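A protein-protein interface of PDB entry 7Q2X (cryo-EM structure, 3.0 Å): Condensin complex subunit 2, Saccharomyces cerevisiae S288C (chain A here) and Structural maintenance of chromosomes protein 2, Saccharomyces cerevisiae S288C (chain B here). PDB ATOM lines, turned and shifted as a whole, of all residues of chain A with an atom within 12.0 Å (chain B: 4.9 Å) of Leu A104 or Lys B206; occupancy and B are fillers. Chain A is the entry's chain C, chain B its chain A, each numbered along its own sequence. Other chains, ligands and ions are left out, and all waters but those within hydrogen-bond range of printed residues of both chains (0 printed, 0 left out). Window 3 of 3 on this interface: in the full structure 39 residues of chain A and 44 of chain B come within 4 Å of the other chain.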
ATOM      1  N   THR A  95       9.006  24.135  -4.544  1.00  0.00           N
ATOM      2  CA  THR A  95       9.421  23.462  -5.773  1.00  0.00           C
ATOM      3  C   THR A  95      10.409  24.308  -6.572  1.00  0.00           C
ATOM      4  O   THR A  95      11.306  23.755  -7.219  1.00  0.00           O
ATOM      5  CB  THR A  95       8.203  23.075  -6.622  1.00  0.00           C
ATOM      6  OG1 THR A  95       8.609  22.162  -7.649  1.00  0.00           O
ATOM      7  CG2 THR A  95       7.555  24.286  -7.269  1.00  0.00           C
ATOM      8  N   GLU A  96      10.289  25.640  -6.523  1.00  0.00           N
ATOM      9  CA  GLU A  96      11.292  26.493  -7.155  1.00  0.00           C
ATOM     10  C   GLU A  96      12.651  26.320  -6.488  1.00  0.00           C
ATOM     11  O   GLU A  96      13.683  26.249  -7.169  1.00  0.00           O
ATOM     12  CB  GLU A  96      10.858  27.959  -7.096  1.00  0.00           C
ATOM     13  CG  GLU A  96       9.679  28.355  -7.987  1.00  0.00           C
ATOM     14  CD  GLU A  96       9.849  27.952  -9.439  1.00  0.00           C
ATOM     15  OE1 GLU A  96      10.236  28.816 -10.254  1.00  0.00           O
ATOM     16  OE2 GLU A  96       9.560  26.786  -9.776  1.00  0.00           O
ATOM     17  N   THR A  97      12.668  26.252  -5.154  1.00  0.00           N
ATOM     18  CA  THR A  97      13.916  26.012  -4.440  1.00  0.00           C
ATOM     19  C   THR A  97      14.499  24.653  -4.800  1.00  0.00           C
ATOM     20  O   THR A  97      15.716  24.516  -4.972  1.00  0.00           O
ATOM     21  CB  THR A  97      13.689  26.116  -2.931  1.00  0.00           C
ATOM     22  OG1 THR A  97      13.174  27.414  -2.612  1.00  0.00           O
ATOM     23  CG2 THR A  97      14.994  25.901  -2.178  1.00  0.00           C
ATOM     24  N   GLY A  98      13.646  23.634  -4.916  1.00  0.00           N
ATOM     25  CA  GLY A  98      14.124  22.327  -5.338  1.00  0.00           C
ATOM     26  C   GLY A  98      14.734  22.346  -6.726  1.00  0.00           C
ATOM     27  O   GLY A  98      15.786  21.744  -6.962  1.00  0.00           O
ATOM     28  N   LYS A  99      14.085  23.041  -7.665  1.00  0.00           N
ATOM     29  CA  LYS A  99      14.642  23.165  -9.010  1.00  0.00           C
ATOM     30  C   LYS A  99      15.989  23.874  -8.985  1.00  0.00           C
ATOM     31  O   LYS A  99      16.929  23.464  -9.677  1.00  0.00           O
ATOM     32  CB  LYS A  99      13.677  23.918  -9.928  1.00  0.00           C
ATOM     33  CG  LYS A  99      12.365  23.217 -10.216  1.00  0.00           C
ATOM     34  CD  LYS A  99      11.250  24.242 -10.352  1.00  0.00           C
ATOM     35  CE  LYS A  99       9.961  23.629 -10.863  1.00  0.00           C
ATOM     36  NZ  LYS A  99       9.801  23.819 -12.331  1.00  0.00           N
ATOM     37  N   LEU A 100      16.100  24.950  -8.202  1.00  0.00           N
ATOM     38  CA  LEU A 100      17.358  25.689  -8.139  1.00  0.00           C
ATOM     39  C   LEU A 100      18.466  24.837  -7.529  1.00  0.00           C
ATOM     40  O   LEU A 100      19.612  24.865  -7.992  1.00  0.00           O
ATOM     41  CB  LEU A 100      17.166  26.984  -7.350  1.00  0.00           C
ATOM     42  CG  LEU A 100      18.224  28.067  -7.572  1.00  0.00           C
ATOM     43  CD1 LEU A 100      18.572  28.182  -9.046  1.00  0.00           C
ATOM     44  CD2 LEU A 100      17.739  29.403  -7.040  1.00  0.00           C
ATOM     45  N   LEU A 101      18.140  24.069  -6.487  1.00  0.00           N
ATOM     46  CA  LEU A 101      19.130  23.180  -5.884  1.00  0.00           C
ATOM     47  C   LEU A 101      19.571  22.101  -6.863  1.00  0.00           C
ATOM     48  O   LEU A 101      20.758  21.762  -6.930  1.00  0.00           O
ATOM     49  CB  LEU A 101      18.567  22.546  -4.613  1.00  0.00           C
ATOM     50  CG  LEU A 101      18.308  23.475  -3.428  1.00  0.00           C
ATOM     51  CD1 LEU A 101      17.245  22.874  -2.528  1.00  0.00           C
ATOM     52  CD2 LEU A 101      19.589  23.734  -2.655  1.00  0.00           C
ATOM     53  N   SER A 102      18.628  21.540  -7.625  1.00  0.00           N
ATOM     54  CA  SER A 102      18.991  20.551  -8.634  1.00  0.00           C
ATOM     55  C   SER A 102      19.883  21.163  -9.706  1.00  0.00           C
ATOM     56  O   SER A 102      20.827  20.522 -10.182  1.00  0.00           O
ATOM     57  CB  SER A 102      17.733  19.949  -9.259  1.00  0.00           C
ATOM     58  OG  SER A 102      16.997  19.207  -8.303  1.00  0.00           O
ATOM     59  N   GLY A 103      19.594  22.403 -10.103  1.00  0.00           N
ATOM     60  CA  GLY A 103      20.448  23.079 -11.066  1.00  0.00           C
ATOM     61  C   GLY A 103      21.841  23.343 -10.525  1.00  0.00           C
ATOM     62  O   GLY A 103      22.826  23.282 -11.267  1.00  0.00           O
ATOM     63  N   LEU A 104      21.943  23.642  -9.232  1.00  0.00           N
ATOM     64  CA  LEU A 104      23.226  23.882  -8.586  1.00  0.00           C
ATOM     65  C   LEU A 104      23.847  22.620  -8.001  1.00  0.00           C
ATOM     66  O   LEU A 104      24.911  22.702  -7.380  1.00  0.00           O
ATOM     67  CB  LEU A 104      23.073  24.933  -7.481  1.00  0.00           C
ATOM     68  CG  LEU A 104      22.708  26.347  -7.934  1.00  0.00           C
ATOM     69  CD1 LEU A 104      22.452  27.242  -6.735  1.00  0.00           C
ATOM     70  CD2 LEU A 104      23.815  26.918  -8.804  1.00  0.00           C
ATOM     71  N   ALA A 105      23.212  21.460  -8.179  1.00  0.00           N
ATOM     72  CA  ALA A 105      23.758  20.213  -7.658  1.00  0.00           C
ATOM     73  C   ALA A 105      25.025  19.773  -8.378  1.00  0.00           C
ATOM     74  O   ALA A 105      25.783  18.972  -7.823  1.00  0.00           O
ATOM     75  CB  ALA A 105      22.708  19.106  -7.739  1.00  0.00           C
ATOM     76  N   GLN A 106      25.272  20.268  -9.586  1.00  0.00           N
ATOM     77  CA  GLN A 106      26.474  19.908 -10.330  1.00  0.00           C
ATOM     78  C   GLN A 106      27.263  21.150 -10.732  1.00  0.00           C
ATOM     79  O   GLN A 106      28.351  21.049 -11.297  1.00  0.00           O
ATOM     80  CB  GLN A 106      26.116  19.090 -11.573  1.00  0.00           C
ATOM     81  CG  GLN A 106      25.242  17.880 -11.290  1.00  0.00           C
ATOM     82  CD  GLN A 106      24.445  17.442 -12.503  1.00  0.00           C
ATOM     83  OE1 GLN A 106      23.457  16.720 -12.383  1.00  0.00           O
ATOM     84  NE2 GLN A 106      24.873  17.880 -13.682  1.00  0.00           N
ATOM     85  N   GLU B 202      22.702  26.740   1.469  1.00  0.00           N
ATOM     86  CA  GLU B 202      23.157  26.022   0.283  1.00  0.00           C
ATOM     87  C   GLU B 202      23.659  26.975  -0.801  1.00  0.00           C
ATOM     88  O   GLU B 202      24.803  26.860  -1.252  1.00  0.00           O
ATOM     89  CB  GLU B 202      22.030  25.135  -0.259  1.00  0.00           C
ATOM     90  CG  GLU B 202      21.709  23.935   0.618  1.00  0.00           C
ATOM     91  CD  GLU B 202      22.843  22.928   0.672  1.00  0.00           C
ATOM     92  OE1 GLU B 202      23.600  22.829  -0.317  1.00  0.00           O
ATOM     93  OE2 GLU B 202      22.977  22.238   1.703  1.00  0.00           O
ATOM     94  N   ILE B 203      22.815  27.916  -1.228  1.00  0.00           N
ATOM     95  CA  ILE B 203      23.142  28.745  -2.381  1.00  0.00           C
ATOM     96  C   ILE B 203      24.266  29.723  -2.060  1.00  0.00           C
ATOM     97  O   ILE B 203      25.186  29.901  -2.865  1.00  0.00           O
ATOM     98  CB  ILE B 203      21.883  29.473  -2.884  1.00  0.00           C
ATOM     99  CG1 ILE B 203      20.772  28.462  -3.175  1.00  0.00           C
ATOM    100  CG2 ILE B 203      22.203  30.300  -4.121  1.00  0.00           C
ATOM    101  CD1 ILE B 203      19.635  29.021  -3.993  1.00  0.00           C
ATOM    102  N   GLU B 204      24.211  30.384  -0.896  1.00  0.00           N
ATOM    103  CA  GLU B 204      25.176  31.448  -0.620  1.00  0.00           C
ATOM    104  C   GLU B 204      26.623  30.974  -0.704  1.00  0.00           C
ATOM    105  O   GLU B 204      27.432  31.657  -1.359  1.00  0.00           O
ATOM    106  CB  GLU B 204      24.865  32.090   0.736  1.00  0.00           C
ATOM    107  CG  GLU B 204      23.502  32.761   0.802  1.00  0.00           C
ATOM    108  CD  GLU B 204      23.272  33.734  -0.339  1.00  0.00           C
ATOM    109  OE1 GLU B 204      24.174  34.551  -0.619  1.00  0.00           O
ATOM    110  OE2 GLU B 204      22.188  33.679  -0.957  1.00  0.00           O
ATOM    111  N   PRO B 205      27.026  29.850  -0.093  1.00  0.00           N
ATOM    112  CA  PRO B 205      28.382  29.344  -0.374  1.00  0.00           C
ATOM    113  C   PRO B 205      28.592  29.005  -1.839  1.00  0.00           C
ATOM    114  O   PRO B 205      29.645  29.325  -2.404  1.00  0.00           O
ATOM    115  CB  PRO B 205      28.488  28.103   0.523  1.00  0.00           C
ATOM    116  CG  PRO B 205      27.467  28.305   1.584  1.00  0.00           C
ATOM    117  CD  PRO B 205      26.340  29.025   0.918  1.00  0.00           C
ATOM    118  N   LYS B 206      27.600  28.382  -2.480  1.00  0.00           N
ATOM    119  CA  LYS B 206      27.717  28.080  -3.903  1.00  0.00           C
ATOM    120  C   LYS B 206      27.761  29.355  -4.736  1.00  0.00           C
ATOM    121  O   LYS B 206      28.531  29.447  -5.700  1.00  0.00           O
ATOM    122  CB  LYS B 206      26.559  27.186  -4.346  1.00  0.00           C
ATOM    123  CG  LYS B 206      26.604  25.785  -3.756  1.00  0.00           C
ATOM    124  CD  LYS B 206      25.328  25.016  -4.056  1.00  0.00           C
ATOM    125  CE  LYS B 206      25.256  23.734  -3.244  1.00  0.00           C
ATOM    126  NZ  LYS B 206      26.289  22.748  -3.670  1.00  0.00           N
ATOM    127  N   LEU B 207      26.943  30.348  -4.380  1.00  0.00           N
ATOM    128  CA  LEU B 207      26.946  31.609  -5.115  1.00  0.00           C
ATOM    129  C   LEU B 207      28.293  32.310  -5.003  1.00  0.00           C
ATOM    130  O   LEU B 207      28.822  32.815  -6.001  1.00  0.00           O
ATOM    131  CB  LEU B 207      25.826  32.517  -4.608  1.00  0.00           C
ATOM    132  CG  LEU B 207      25.402  33.652  -5.541  1.00  0.00           C
ATOM    133  CD1 LEU B 207      25.048  33.112  -6.919  1.00  0.00           C
ATOM    134  CD2 LEU B 207      24.237  34.429  -4.948  1.00  0.00           C
ATOM    135  N   GLU B 208      28.873  32.344  -3.800  1.00  0.00           N
ATOM    136  CA  GLU B 208      30.170  32.996  -3.648  1.00  0.00           C
ATOM    137  C   GLU B 208      31.279  32.200  -4.326  1.00  0.00           C
ATOM    138  O   GLU B 208      32.223  32.794  -4.859  1.00  0.00           O
ATOM    139  CB  GLU B 208      30.484  33.231  -2.167  1.00  0.00           C
ATOM    140  CG  GLU B 208      30.837  31.990  -1.367  1.00  0.00           C
ATOM    141  CD  GLU B 208      31.100  32.296   0.094  1.00  0.00           C
ATOM    142  OE1 GLU B 208      31.740  33.329   0.381  1.00  0.00           O
ATOM    143  OE2 GLU B 208      30.668  31.502   0.955  1.00  0.00           O
ATOM    144  N   LYS B 209      31.178  30.866  -4.342  1.00  0.00           N
ATOM    145  CA  LYS B 209      32.150  30.067  -5.083  1.00  0.00           C
ATOM    146  C   LYS B 209      32.076  30.358  -6.577  1.00  0.00           C
ATOM    147  O   LYS B 209      33.109  30.488  -7.245  1.00  0.00           O
ATOM    148  CB  LYS B 209      31.921  28.580  -4.812  1.00  0.00           C
ATOM    149  CG  LYS B 209      32.448  28.107  -3.468  1.00  0.00           C
ATOM    150  CD  LYS B 209      32.155  26.632  -3.248  1.00  0.00           C
ATOM    151  CE  LYS B 209      32.770  26.136  -1.949  1.00  0.00           C
ATOM    152  NZ  LYS B 209      31.734  25.845  -0.922  1.00  0.00           N
ATOM    153  N   LEU B 210      30.861  30.464  -7.120  1.00  0.00           N
ATOM    154  CA  LEU B 210      30.710  30.792  -8.536  1.00  0.00           C
ATOM    155  C   LEU B 210      31.227  32.194  -8.836  1.00  0.00           C
ATOM    156  O   LEU B 210      31.868  32.421  -9.869  1.00  0.00           O
ATOM    157  CB  LEU B 210      29.247  30.651  -8.953  1.00  0.00           C
ATOM    158  CG  LEU B 210      28.688  29.227  -8.907  1.00  0.00           C
ATOM    159  CD1 LEU B 210      27.197  29.212  -9.202  1.00  0.00           C
ATOM    160  CD2 LEU B 210      29.438  28.326  -9.876  1.00  0.00           C
ATOM    161  N   VAL B 993      20.622  31.250 -12.810  1.00  0.00           N
ATOM    162  CA  VAL B 993      20.589  31.148 -11.354  1.00  0.00           C
ATOM    163  C   VAL B 993      20.244  32.494 -10.733  1.00  0.00           C
ATOM    164  O   VAL B 993      19.467  32.571  -9.774  1.00  0.00           O
ATOM    165  CB  VAL B 993      21.931  30.600 -10.831  1.00  0.00           C
ATOM    166  CG1 VAL B 993      22.105  30.915  -9.352  1.00  0.00           C
ATOM    167  CG2 VAL B 993      22.020  29.105 -11.077  1.00  0.00           C
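Leu A100 touches Ile B203. CD2 of Leu A101 touches CB of Glu B202, at 3.7 Å. O of Leu A104 touches NZ of Lys B206, at 3.96 Å. CD2 of Leu A104 touches CG2 of Val B993, at 3.6 Å.
Glu B202 touches one residue of chain A. Ile B203 touches just one residue of chain A: Leu A100. No residue of chain A comes within 4 Å of Glu B204. Leu B207 touches none of the printed residues of chain A. Of chain A, only Leu A104 comes within 4 Å of Val B993. Printed residues of chain B within 4 Å of Leu A100: Ile B203 (3.6 Å). Of the printed residues of chain B, Leu A101 touches Glu B202 (3.7 Å). The nearest residue of chain B that does not touch Leu A104 is Ile B203 (4.03 Å). The nearest residue of chain A that does not touch Lys B206 is Ala A105 (5.4 Å).
Hydrophobic or aromatic side chains of chain B that line the printed part of chain A: Ile B203 and Val B993. Printed residues of chain A that touch a printed residue of chain B: Leu A100, Leu A101 and Leu A104. Among the printed residues, 4 pairs touch across the chains. Among the printed residues, no Asp or Glu carboxylate lies within 4 Å of a Lys or Arg side-chain nitrogen of the other chain.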
